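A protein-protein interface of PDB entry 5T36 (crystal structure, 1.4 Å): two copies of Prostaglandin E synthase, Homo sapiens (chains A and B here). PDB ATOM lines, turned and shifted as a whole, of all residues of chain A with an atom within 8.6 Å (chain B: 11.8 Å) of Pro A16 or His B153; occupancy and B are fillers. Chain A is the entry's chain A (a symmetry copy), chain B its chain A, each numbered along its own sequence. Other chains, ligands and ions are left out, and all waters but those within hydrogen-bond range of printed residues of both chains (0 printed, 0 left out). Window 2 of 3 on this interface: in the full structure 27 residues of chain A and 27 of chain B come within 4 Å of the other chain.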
ATOM      1  N   LEU A   8      25.126   3.405 -21.229  1.00  0.00           N
ATOM      2  CA  LEU A   8      24.673   2.580 -20.070  1.00  0.00           C
ATOM      3  C   LEU A   8      24.994   3.280 -18.748  1.00  0.00           C
ATOM      4  O   LEU A   8      25.928   4.082 -18.670  1.00  0.00           O
ATOM      5  CB  LEU A   8      25.310   1.186 -20.131  1.00  0.00           C
ATOM      6  CG  LEU A   8      24.565   0.010 -19.486  1.00  0.00           C
ATOM      7  CD1 LEU A   8      24.639  -1.225 -20.375  1.00  0.00           C
ATOM      8  CD2 LEU A   8      25.092  -0.296 -18.091  1.00  0.00           C
ATOM      9  N   VAL A   9      24.211   2.967 -17.717  1.00  0.00           N
ATOM     10  CA  VAL A   9      24.314   3.609 -16.399  1.00  0.00           C
ATOM     11  C   VAL A   9      25.635   3.300 -15.679  1.00  0.00           C
ATOM     12  O   VAL A   9      26.085   4.077 -14.832  1.00  0.00           O
ATOM     13  CB  VAL A   9      23.096   3.238 -15.503  1.00  0.00           C
ATOM     14  CG1 VAL A   9      23.136   3.970 -14.171  1.00  0.00           C
ATOM     15  CG2 VAL A   9      21.795   3.558 -16.221  1.00  0.00           C
ATOM     16  N   MET A  10      26.260   2.179 -16.032  1.00  0.00           N
ATOM     17  CA  MET A  10      27.518   1.758 -15.412  1.00  0.00           C
ATOM     18  C   MET A  10      28.765   2.228 -16.177  1.00  0.00           C
ATOM     19  O   MET A  10      29.842   1.641 -16.040  1.00  0.00           O
ATOM     20  CB  MET A  10      27.539   0.235 -15.232  1.00  0.00           C
ATOM     21  N   SER A  11      28.612   3.290 -16.969  1.00  0.00           N
ATOM     22  CA  SER A  11      29.723   3.874 -17.728  1.00  0.00           C
ATOM     23  C   SER A  11      30.788   4.483 -16.813  1.00  0.00           C
ATOM     24  O   SER A  11      31.956   4.597 -17.194  1.00  0.00           O
ATOM     25  CB  SER A  11      29.209   4.927 -18.713  1.00  0.00           C
ATOM     26  OG  SER A  11      28.392   4.336 -19.710  1.00  0.00           O
ATOM     27  N   SER A  12      30.367   4.875 -15.612  1.00  0.00           N
ATOM     28  CA  SER A  12      31.261   5.363 -14.566  1.00  0.00           C
ATOM     29  C   SER A  12      30.657   5.044 -13.195  1.00  0.00           C
ATOM     30  O   SER A  12      29.432   5.032 -13.052  1.00  0.00           O
ATOM     31  CB  SER A  12      31.500   6.867 -14.716  1.00  0.00           C
ATOM     32  OG  SER A  12      30.292   7.597 -14.605  1.00  0.00           O
ATOM     33  N   PRO A  13      31.511   4.781 -12.181  1.00  0.00           N
ATOM     34  CA  PRO A  13      31.040   4.396 -10.844  1.00  0.00           C
ATOM     35  C   PRO A  13      30.111   5.412 -10.167  1.00  0.00           C
ATOM     36  O   PRO A  13      29.269   5.024  -9.356  1.00  0.00           O
ATOM     37  CB  PRO A  13      32.338   4.261 -10.040  1.00  0.00           C
ATOM     38  CG  PRO A  13      33.375   3.956 -11.056  1.00  0.00           C
ATOM     39  CD  PRO A  13      32.984   4.746 -12.266  1.00  0.00           C
ATOM     40  N   ALA A  14      30.262   6.690 -10.508  1.00  0.00           N
ATOM     41  CA  ALA A  14      29.482   7.761  -9.884  1.00  0.00           C
ATOM     42  C   ALA A  14      28.148   8.036 -10.580  1.00  0.00           C
ATOM     43  O   ALA A  14      27.271   8.692 -10.011  1.00  0.00           O
ATOM     44  CB  ALA A  14      30.313   9.037  -9.810  1.00  0.00           C
ATOM     45  N   LEU A  15      27.998   7.526 -11.802  1.00  0.00           N
ATOM     46  CA  LEU A  15      26.834   7.832 -12.644  1.00  0.00           C
ATOM     47  C   LEU A  15      25.467   7.419 -12.069  1.00  0.00           C
ATOM     48  O   LEU A  15      24.530   8.216 -12.120  1.00  0.00           O
ATOM     49  CB  LEU A  15      27.021   7.291 -14.072  1.00  0.00           C
ATOM     50  CG  LEU A  15      26.061   7.780 -15.164  1.00  0.00           C
ATOM     51  CD1 LEU A  15      26.164   9.290 -15.379  1.00  0.00           C
ATOM     52  CD2 LEU A  15      26.313   7.040 -16.466  1.00  0.00           C
ATOM     53  N   PRO A  16      25.337   6.183 -11.530  1.00  0.00           N
ATOM     54  CA  PRO A  16      24.035   5.802 -10.966  1.00  0.00           C
ATOM     55  C   PRO A  16      23.547   6.753  -9.870  1.00  0.00           C
ATOM     56  O   PRO A  16      22.369   7.120  -9.858  1.00  0.00           O
ATOM     57  CB  PRO A  16      24.294   4.405 -10.391  1.00  0.00           C
ATOM     58  CG  PRO A  16      25.415   3.875 -11.194  1.00  0.00           C
ATOM     59  CD  PRO A  16      26.289   5.055 -11.491  1.00  0.00           C
ATOM     60  N   ALA A  17      24.452   7.152  -8.976  1.00  0.00           N
ATOM     61  CA  ALA A  17      24.126   8.085  -7.896  1.00  0.00           C
ATOM     62  C   ALA A  17      23.709   9.447  -8.440  1.00  0.00           C
ATOM     63  O   ALA A  17      22.758  10.052  -7.938  1.00  0.00           O
ATOM     64  CB  ALA A  17      25.299   8.232  -6.943  1.00  0.00           C
ATOM     65  N   PHE A  18      24.421   9.924  -9.460  1.00  0.00           N
ATOM     66  CA  PHE A  18      24.068  11.184 -10.106  1.00  0.00           C
ATOM     67  C   PHE A  18      22.681  11.120 -10.730  1.00  0.00           C
ATOM     68  O   PHE A  18      21.874  12.033 -10.550  1.00  0.00           O
ATOM     69  CB  PHE A  18      25.091  11.598 -11.169  1.00  0.00           C
ATOM     70  CG  PHE A  18      24.587  12.680 -12.087  1.00  0.00           C
ATOM     71  CD1 PHE A  18      24.481  13.994 -11.640  1.00  0.00           C
ATOM     72  CD2 PHE A  18      24.182  12.378 -13.384  1.00  0.00           C
ATOM     73  CE1 PHE A  18      23.994  14.992 -12.477  1.00  0.00           C
ATOM     74  CE2 PHE A  18      23.691  13.369 -14.228  1.00  0.00           C
ATOM     75  CZ  PHE A  18      23.600  14.680 -13.774  1.00  0.00           C
ATOM     76  N   LEU A  19      22.414  10.046 -11.471  1.00  0.00           N
ATOM     77  CA  LEU A  19      21.142   9.889 -12.172  1.00  0.00           C
ATOM     78  C   LEU A  19      19.962   9.772 -11.210  1.00  0.00           C
ATOM     79  O   LEU A  19      18.881  10.292 -11.486  1.00  0.00           O
ATOM     80  CB  LEU A  19      21.186   8.706 -13.146  1.00  0.00           C
ATOM     81  CG  LEU A  19      22.120   8.839 -14.357  1.00  0.00           C
ATOM     82  CD1 LEU A  19      22.145   7.549 -15.164  1.00  0.00           C
ATOM     83  CD2 LEU A  19      21.742  10.022 -15.244  1.00  0.00           C
ATOM     84  N   LEU A  20      20.184   9.108 -10.075  1.00  0.00           N
ATOM     85  CA  LEU A  20      19.169   9.001  -9.028  1.00  0.00           C
ATOM     86  C   LEU A  20      18.819  10.379  -8.464  1.00  0.00           C
ATOM     87  O   LEU A  20      17.648  10.763  -8.440  1.00  0.00           O
ATOM     88  CB  LEU A  20      19.645   8.068  -7.907  1.00  0.00           C
ATOM     89  CG  LEU A  20      18.654   7.714  -6.793  1.00  0.00           C
ATOM     90  CD1 LEU A  20      17.769   6.543  -7.196  1.00  0.00           C
ATOM     91  CD2 LEU A  20      19.400   7.394  -5.506  1.00  0.00           C
ATOM     92  N   CYS A  21      19.839  11.118  -8.027  1.00  0.00           N
ATOM     93  CA  CYS A  21      19.648  12.431  -7.410  1.00  0.00           C
ATOM     94  C   CYS A  21      19.050  13.450  -8.377  1.00  0.00           C
ATOM     95  O   CYS A  21      18.135  14.190  -8.015  1.00  0.00           O
ATOM     96  CB  CYS A  21      20.966  12.953  -6.834  1.00  0.00           C
ATOM     97  SG  CYS A  21      21.572  12.009  -5.418  1.00  0.00           S
ATOM     98  N   SER A  22      19.561  13.468  -9.607  1.00  0.00           N
ATOM     99  CA  SER A  22      19.096  14.408 -10.627  1.00  0.00           C
ATOM    100  C   SER A  22      17.643  14.173 -11.020  1.00  0.00           C
ATOM    101  O   SER A  22      16.868  15.123 -11.131  1.00  0.00           O
ATOM    102  CB  SER A  22      20.003  14.361 -11.858  1.00  0.00           C
ATOM    103  OG  SER A  22      20.092  13.048 -12.380  1.00  0.00           O
ATOM    104  N   THR A  23      17.278  12.908 -11.223  1.00  0.00           N
ATOM    105  CA  THR A  23      15.917  12.562 -11.628  1.00  0.00           C
ATOM    106  C   THR A  23      14.919  12.850 -10.505  1.00  0.00           C
ATOM    107  O   THR A  23      13.815  13.329 -10.765  1.00  0.00           O
ATOM    108  CB  THR A  23      15.817  11.101 -12.113  1.00  0.00           C
ATOM    109  OG1 THR A  23      16.802  10.873 -13.129  1.00  0.00           O
ATOM    110  CG2 THR A  23      14.444  10.815 -12.693  1.00  0.00           C
ATOM    111  N   SER A  92      30.619  13.204 -13.259  1.00  0.00           N
ATOM    112  CA  SER A  92      30.526  11.746 -13.123  1.00  0.00           C
ATOM    113  C   SER A  92      31.548  11.000 -13.986  1.00  0.00           C
ATOM    114  O   SER A  92      31.961   9.891 -13.639  1.00  0.00           O
ATOM    115  CB  SER A  92      29.112  11.261 -13.451  1.00  0.00           C
ATOM    116  OG  SER A  92      28.180  11.709 -12.483  1.00  0.00           O
ATOM    117  N   PHE A  93      31.954  11.614 -15.098  1.00  0.00           N
ATOM    118  CA  PHE A  93      32.889  10.993 -16.041  1.00  0.00           C
ATOM    119  C   PHE A  93      34.347  11.428 -15.860  1.00  0.00           C
ATOM    120  O   PHE A  93      35.216  11.045 -16.652  1.00  0.00           O
ATOM    121  CB  PHE A  93      32.436  11.243 -17.484  1.00  0.00           C
ATOM    122  CG  PHE A  93      31.191  10.494 -17.871  1.00  0.00           C
ATOM    123  CD1 PHE A  93      31.265   9.175 -18.307  1.00  0.00           C
ATOM    124  CD2 PHE A  93      29.946  11.107 -17.803  1.00  0.00           C
ATOM    125  CE1 PHE A  93      30.114   8.476 -18.667  1.00  0.00           C
ATOM    126  CE2 PHE A  93      28.789  10.418 -18.159  1.00  0.00           C
ATOM    127  CZ  PHE A  93      28.874   9.100 -18.592  1.00  0.00           C
ATOM    128  N   TRP A 102      29.396  10.895  -4.343  1.00  0.00           N
ATOM    129  CA  TRP A 102      28.133  10.648  -3.648  1.00  0.00           C
ATOM    130  C   TRP A 102      27.776  11.792  -2.700  1.00  0.00           C
ATOM    131  O   TRP A 102      26.623  12.227  -2.661  1.00  0.00           O
ATOM    132  CB  TRP A 102      28.194   9.324  -2.877  1.00  0.00           C
ATOM    133  CG  TRP A 102      27.905   8.096  -3.706  1.00  0.00           C
ATOM    134  CD1 TRP A 102      28.325   7.843  -4.983  1.00  0.00           C
ATOM    135  CD2 TRP A 102      27.151   6.946  -3.301  1.00  0.00           C
ATOM    136  NE1 TRP A 102      27.873   6.616  -5.400  1.00  0.00           N
ATOM    137  CE2 TRP A 102      27.149   6.042  -4.388  1.00  0.00           C
ATOM    138  CE3 TRP A 102      26.470   6.592  -2.128  1.00  0.00           C
ATOM    139  CZ2 TRP A 102      26.493   4.807  -4.338  1.00  0.00           C
ATOM    140  CZ3 TRP A 102      25.819   5.362  -2.077  1.00  0.00           C
ATOM    141  CH2 TRP A 102      25.837   4.486  -3.177  1.00  0.00           C
ATOM    142  N   PHE A 105      26.566  14.908  -4.620  1.00  0.00           N
ATOM    143  CA  PHE A 105      25.195  14.751  -5.104  1.00  0.00           C
ATOM    144  C   PHE A 105      24.166  14.791  -3.974  1.00  0.00           C
ATOM    145  O   PHE A 105      23.099  15.391  -4.131  1.00  0.00           O
ATOM    146  CB  PHE A 105      25.030  13.457  -5.919  1.00  0.00           C
ATOM    147  CG  PHE A 105      26.036  13.290  -7.036  1.00  0.00           C
ATOM    148  CD1 PHE A 105      26.477  14.381  -7.784  1.00  0.00           C
ATOM    149  CD2 PHE A 105      26.516  12.023  -7.359  1.00  0.00           C
ATOM    150  CE1 PHE A 105      27.401  14.213  -8.817  1.00  0.00           C
ATOM    151  CE2 PHE A 105      27.436  11.847  -8.388  1.00  0.00           C
ATOM    152  CZ  PHE A 105      27.879  12.941  -9.119  1.00  0.00           C
ATOM    153  N   PHE B  86      17.362  16.682 -20.665  1.00  0.00           N
ATOM    154  CA  PHE B  86      18.095  15.798 -19.767  1.00  0.00           C
ATOM    155  C   PHE B  86      17.508  14.384 -19.749  1.00  0.00           C
ATOM    156  O   PHE B  86      18.224  13.411 -20.000  1.00  0.00           O
ATOM    157  CB  PHE B  86      18.141  16.379 -18.348  1.00  0.00           C
ATOM    158  CG  PHE B  86      18.819  15.482 -17.351  1.00  0.00           C
ATOM    159  CD1 PHE B  86      20.208  15.401 -17.300  1.00  0.00           C
ATOM    160  CD2 PHE B  86      18.070  14.707 -16.471  1.00  0.00           C
ATOM    161  CE1 PHE B  86      20.841  14.565 -16.387  1.00  0.00           C
ATOM    162  CE2 PHE B  86      18.694  13.867 -15.552  1.00  0.00           C
ATOM    163  CZ  PHE B  86      20.083  13.798 -15.513  1.00  0.00           C
ATOM    164  N   VAL B  90      19.262  10.726 -21.361  1.00  0.00           N
ATOM    165  CA  VAL B  90      19.557   9.579 -20.501  1.00  0.00           C
ATOM    166  C   VAL B  90      18.717   8.364 -20.911  1.00  0.00           C
ATOM    167  O   VAL B  90      19.240   7.254 -21.042  1.00  0.00           O
ATOM    168  CB  VAL B  90      19.334   9.925 -19.004  1.00  0.00           C
ATOM    169  CG1 VAL B  90      19.561   8.705 -18.117  1.00  0.00           C
ATOM    170  CG2 VAL B  90      20.245  11.073 -18.578  1.00  0.00           C
ATOM    171  N   PHE B  93      19.743   6.034 -23.767  1.00  0.00           N
ATOM    172  CA  PHE B  93      20.824   5.082 -23.494  1.00  0.00           C
ATOM    173  C   PHE B  93      20.428   3.931 -22.563  1.00  0.00           C
ATOM    174  O   PHE B  93      21.275   3.115 -22.185  1.00  0.00           O
ATOM    175  CB  PHE B  93      22.053   5.814 -22.940  1.00  0.00           C
ATOM    176  CG  PHE B  93      22.757   6.674 -23.952  1.00  0.00           C
ATOM    177  CD1 PHE B  93      23.693   6.122 -24.821  1.00  0.00           C
ATOM    178  CD2 PHE B  93      22.488   8.034 -24.035  1.00  0.00           C
ATOM    179  CE1 PHE B  93      24.349   6.915 -25.761  1.00  0.00           C
ATOM    180  CE2 PHE B  93      23.137   8.837 -24.970  1.00  0.00           C
ATOM    181  CZ  PHE B  93      24.069   8.275 -25.835  1.00  0.00           C
ATOM    182  N   LEU B  94      19.149   3.861 -22.205  1.00  0.00           N
ATOM    183  CA  LEU B  94      18.645   2.795 -21.331  1.00  0.00           C
ATOM    184  C   LEU B  94      18.167   1.575 -22.120  1.00  0.00           C
ATOM    185  O   LEU B  94      17.655   0.612 -21.542  1.00  0.00           O
ATOM    186  CB  LEU B  94      17.519   3.315 -20.428  1.00  0.00           C
ATOM    187  CG  LEU B  94      17.758   4.519 -19.510  1.00  0.00           C
ATOM    188  CD1 LEU B  94      16.503   4.796 -18.702  1.00  0.00           C
ATOM    189  CD2 LEU B  94      18.954   4.321 -18.588  1.00  0.00           C
ATOM    190  N   GLY B  95      18.346   1.626 -23.438  1.00  0.00           N
ATOM    191  CA  GLY B  95      17.911   0.561 -24.341  1.00  0.00           C
ATOM    192  C   GLY B  95      16.407   0.340 -24.371  1.00  0.00           C
ATOM    193  O   GLY B  95      15.952  -0.796 -24.209  1.00  0.00           O
ATOM    194  N   ALA B 143      11.238   9.643 -16.524  1.00  0.00           N
ATOM    195  CA  ALA B 143      11.785   9.900 -15.190  1.00  0.00           C
ATOM    196  C   ALA B 143      11.736   8.658 -14.300  1.00  0.00           C
ATOM    197  O   ALA B 143      12.731   8.309 -13.668  1.00  0.00           O
ATOM    198  CB  ALA B 143      11.062  11.066 -14.526  1.00  0.00           C
ATOM    199  N   LEU B 144      10.583   7.992 -14.270  1.00  0.00           N
ATOM    200  CA  LEU B 144      10.419   6.772 -13.478  1.00  0.00           C
ATOM    201  C   LEU B 144      11.327   5.644 -13.965  1.00  0.00           C
ATOM    202  O   LEU B 144      11.918   4.930 -13.155  1.00  0.00           O
ATOM    203  CB  LEU B 144       8.954   6.318 -13.455  1.00  0.00           C
ATOM    204  CG  LEU B 144       7.954   7.189 -12.683  1.00  0.00           C
ATOM    205  CD1 LEU B 144       6.532   6.705 -12.922  1.00  0.00           C
ATOM    206  CD2 LEU B 144       8.264   7.223 -11.187  1.00  0.00           C
ATOM    207  N   GLN B 145      11.448   5.498 -15.284  1.00  0.00           N
ATOM    208  CA  GLN B 145      12.310   4.470 -15.873  1.00  0.00           C
ATOM    209  C   GLN B 145      13.780   4.694 -15.525  1.00  0.00           C
ATOM    210  O   GLN B 145      14.505   3.741 -15.232  1.00  0.00           O
ATOM    211  CB  GLN B 145      12.121   4.395 -17.390  1.00  0.00           C
ATOM    212  CG  GLN B 145      10.773   3.832 -17.814  1.00  0.00           C
ATOM    213  CD  GLN B 145      10.608   3.767 -19.320  1.00  0.00           C
ATOM    214  OE1 GLN B 145      11.313   3.024 -20.002  1.00  0.00           O
ATOM    215  NE2 GLN B 145       9.665   4.541 -19.846  1.00  0.00           N
ATOM    216  N   ILE B 146      14.211   5.955 -15.554  1.00  0.00           N
ATOM    217  CA  ILE B 146      15.571   6.322 -15.157  1.00  0.00           C
ATOM    218  C   ILE B 146      15.793   6.042 -13.666  1.00  0.00           C
ATOM    219  O   ILE B 146      16.854   5.541 -13.281  1.00  0.00           O
ATOM    220  CB  ILE B 146      15.900   7.800 -15.504  1.00  0.00           C
ATOM    221  CG1 ILE B 146      15.835   8.016 -17.020  1.00  0.00           C
ATOM    222  CG2 ILE B 146      17.289   8.189 -14.992  1.00  0.00           C
ATOM    223  CD1 ILE B 146      15.712   9.470 -17.447  1.00  0.00           C
ATOM    224  N   LEU B 147      14.785   6.348 -12.845  1.00  0.00           N
ATOM    225  CA  LEU B 147      14.853   6.101 -11.404  1.00  0.00           C
ATOM    226  C   LEU B 147      15.130   4.635 -11.097  1.00  0.00           C
ATOM    227  O   LEU B 147      16.007   4.322 -10.290  1.00  0.00           O
ATOM    228  CB  LEU B 147      13.564   6.531 -10.696  1.00  0.00           C
ATOM    229  CG  LEU B 147      13.321   7.984 -10.282  1.00  0.00           C
ATOM    230  CD1 LEU B 147      12.082   8.035  -9.407  1.00  0.00           C
ATOM    231  CD2 LEU B 147      14.511   8.591  -9.546  1.00  0.00           C
ATOM    232  N   TRP B 148      14.386   3.739 -11.748  1.00  0.00           N
ATOM    233  CA  TRP B 148      14.542   2.300 -11.517  1.00  0.00           C
ATOM    234  C   TRP B 148      15.910   1.796 -11.964  1.00  0.00           C
ATOM    235  O   TRP B 148      16.543   1.009 -11.254  1.00  0.00           O
ATOM    236  CB  TRP B 148      13.442   1.478 -12.206  1.00  0.00           C
ATOM    237  CG  TRP B 148      12.018   1.963 -12.034  1.00  0.00           C
ATOM    238  CD1 TRP B 148      11.015   1.858 -12.954  1.00  0.00           C
ATOM    239  CD2 TRP B 148      11.441   2.617 -10.889  1.00  0.00           C
ATOM    240  NE1 TRP B 148       9.855   2.399 -12.461  1.00  0.00           N
ATOM    241  CE2 TRP B 148      10.086   2.876 -11.198  1.00  0.00           C
ATOM    242  CE3 TRP B 148      11.936   3.012  -9.637  1.00  0.00           C
ATOM    243  CZ2 TRP B 148       9.219   3.511 -10.302  1.00  0.00           C
ATOM    244  CZ3 TRP B 148      11.071   3.646  -8.746  1.00  0.00           C
ATOM    245  CH2 TRP B 148       9.729   3.887  -9.085  1.00  0.00           C
ATOM    246  N   GLU B 149      16.354   2.256 -13.136  1.00  0.00           N
ATOM    247  CA  GLU B 149      17.648   1.861 -13.695  1.00  0.00           C
ATOM    248  C   GLU B 149      18.804   2.359 -12.835  1.00  0.00           C
ATOM    249  O   GLU B 149      19.765   1.630 -12.591  1.00  0.00           O
ATOM    250  CB  GLU B 149      17.803   2.366 -15.134  1.00  0.00           C
ATOM    251  CG  GLU B 149      16.976   1.603 -16.154  1.00  0.00           C
ATOM    252  CD  GLU B 149      17.274   0.118 -16.150  1.00  0.00           C
ATOM    253  OE1 GLU B 149      16.313  -0.680 -16.155  1.00  0.00           O
ATOM    254  OE2 GLU B 149      18.466  -0.253 -16.133  1.00  0.00           O
ATOM    255  N   ALA B 150      18.703   3.607 -12.376  1.00  0.00           N
ATOM    256  CA  ALA B 150      19.728   4.198 -11.516  1.00  0.00           C
ATOM    257  C   ALA B 150      19.782   3.510 -10.151  1.00  0.00           C
ATOM    258  O   ALA B 150      20.861   3.138  -9.683  1.00  0.00           O
ATOM    259  CB  ALA B 150      19.502   5.699 -11.358  1.00  0.00           C
ATOM    260  N   ALA B 151      18.613   3.328  -9.535  1.00  0.00           N
ATOM    261  CA  ALA B 151      18.505   2.704  -8.213  1.00  0.00           C
ATOM    262  C   ALA B 151      19.046   1.276  -8.182  1.00  0.00           C
ATOM    263  O   ALA B 151      19.704   0.883  -7.218  1.00  0.00           O
ATOM    264  CB  ALA B 151      17.061   2.735  -7.721  1.00  0.00           C
ATOM    265  N   ARG B 152      18.779   0.511  -9.240  1.00  0.00           N
ATOM    266  CA  ARG B 152      19.207  -0.890  -9.298  1.00  0.00           C
ATOM    267  C   ARG B 152      20.705  -1.055  -9.579  1.00  0.00           C
ATOM    268  O   ARG B 152      21.256  -2.142  -9.400  1.00  0.00           O
ATOM    269  CB  ARG B 152      18.354  -1.692 -10.294  1.00  0.00           C
ATOM    270  CG  ARG B 152      18.696  -1.498 -11.764  1.00  0.00           C
ATOM    271  CD  ARG B 152      17.739  -2.284 -12.648  1.00  0.00           C
ATOM    272  NE  ARG B 152      18.254  -2.446 -14.007  1.00  0.00           N
ATOM    273  CZ  ARG B 152      19.040  -3.446 -14.403  1.00  0.00           C
ATOM    274  NH1 ARG B 152      19.411  -4.392 -13.549  1.00  0.00           N
ATOM    275  NH2 ARG B 152      19.454  -3.500 -15.662  1.00  0.00           N
ATOM    276  N   HIS B 153      21.352   0.027 -10.010  1.00  0.00           N
ATOM    277  CA  HIS B 153      22.790   0.026 -10.286  1.00  0.00           C
ATOM    278  C   HIS B 153      23.626   0.605  -9.141  1.00  0.00           C
ATOM    279  O   HIS B 153      24.848   0.734  -9.263  1.00  0.00           O
ATOM    280  CB  HIS B 153      23.087   0.771 -11.592  1.00  0.00           C
ATOM    281  CG  HIS B 153      22.870  -0.053 -12.821  1.00  0.00           C
ATOM    282  ND1 HIS B 153      21.662  -0.104 -13.481  1.00  0.00           N
ATOM    283  CD2 HIS B 153      23.709  -0.862 -13.510  1.00  0.00           C
ATOM    284  CE1 HIS B 153      21.765  -0.909 -14.524  1.00  0.00           C
ATOM    285  NE2 HIS B 153      22.997  -1.382 -14.564  1.00  0.00           N
ATOM    286  N   LEU B 154      22.970   0.944  -8.033  1.00  0.00           N
ATOM    287  CA  LEU B 154      23.657   1.496  -6.864  1.00  0.00           C
ATOM    288  C   LEU B 154      24.440   0.424  -6.112  1.00  0.00           C
ATOM    289  O   LEU B 154      23.981  -0.707  -5.954  1.00  0.00           O
ATOM    290  CB  LEU B 154      22.666   2.182  -5.918  1.00  0.00           C
ATOM    291  CG  LEU B 154      21.995   3.484  -6.368  1.00  0.00           C
ATOM    292  CD1 LEU B 154      20.876   3.854  -5.406  1.00  0.00           C
ATOM    293  CD2 LEU B 154      22.998   4.630  -6.490  1.00  0.00           C
ATOM    294  OXT LEU B 154      25.554   0.668  -5.645  1.00  0.00           O
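1 position is printed for both chains.
Of the 20 printed residues of chain A, 9 touch a printed residue of chain B. Printed residues of chain A that touch a printed residue of chain B: Leu A8, Val A9, Pro A16, Ala A17, Phe A18, Leu A19, Leu A20, Ser A22 and Thr A23. Printed residues of chain B that touch a printed residue of chain A: Phe B86, Val B90, Phe B93, Leu B94, Ala B143, Ile B146, Leu B147, Ala B150, Ala B151, His B153 and Leu B154. Among the printed residues, 16 pairs touch across the chains. Among the printed residues, no Asp or Glu carboxylate lies within 4 Å of a Lys or Arg side-chain nitrogen of the other chain.
Of chain B, only Ala B150 (3.5 Å) and His B153 (3.7 Å) come within 4 Å of Pro A16. Met A10 touches none of the printed residues of chain B. No residue of chain B comes within 4 Å of Ser A12. No residue of chain B comes within 4 Å of Pro A13. No residue of chain B comes within 4 Å of Ala A14. Ala A17 touches just one residue of chain B: Leu B154 (3.8 Å). Of chain B, only Val B90 (3.8 Å) and Ala B150 (3.9 Å) come within 4 Å of Leu A19. Of the printed residues of chain B, Leu A8 touches Phe B93 (3.98 Å). Printed residues of chain A within 4 Å of Leu B154: Ala A17 and Leu A20. Printed residues of chain B within 4 Å of Thr A23: Ala B143, Ile B146 and Leu B147. The nearest residue of chain B that does not touch Pro A16 is Leu B154 (4.03 Å).
Among the printed residues, merely in contact across the chains: Thr A23 with Ala B143 (3.2 Å), Ser A22 with Phe B86 (3.2 Å), Thr A23 with Ile B146 (3.3 Å), Pro A16 with Ala B150 (3.5 Å), Leu A20 with Ala B150 (3.7 Å), Pro A16 with His B153 (3.7 Å), Phe A18 with Phe B86 (3.8 Å), Val A9 with Leu B94 (3.8 Å), Leu A19 with Val B90 (3.8 Å), Thr A23 with Leu B147 (3.8 Å), Ala A17 with Leu B154 (3.8 Å), Leu A20 with Leu B154 (3.8 Å), Leu A19 with Ala B150 (3.9 Å), Leu A20 with Ala B151 (3.9 Å), Leu A20 with Leu B147 (3.97 Å) and Leu A8 with Phe B93 (3.98 Å).
O of Glu B149 lies within hydrogen-bond range of ND1 of His B153 (2.7 Å). O of Leu A8 sits at hydrogen-bond distance from OG of Ser A11 (2.7 Å). The side-chain sulfur of Cys A21 sits at hydrogen-bond distance from the backbone carbonyl oxygen of Ala A17, 3.4 Å away. The backbone carbonyl oxygen of Phe A18 lies within hydrogen-bond range of the side-chain hydroxyl of Ser A22, 2.7 Å away. O of Leu A19 is in hydrogen-bond range of OG of Ser A22 (3.1 Å). O of Leu A19 is in hydrogen-bond range of OG1 of Thr A23 (2.7 Å).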
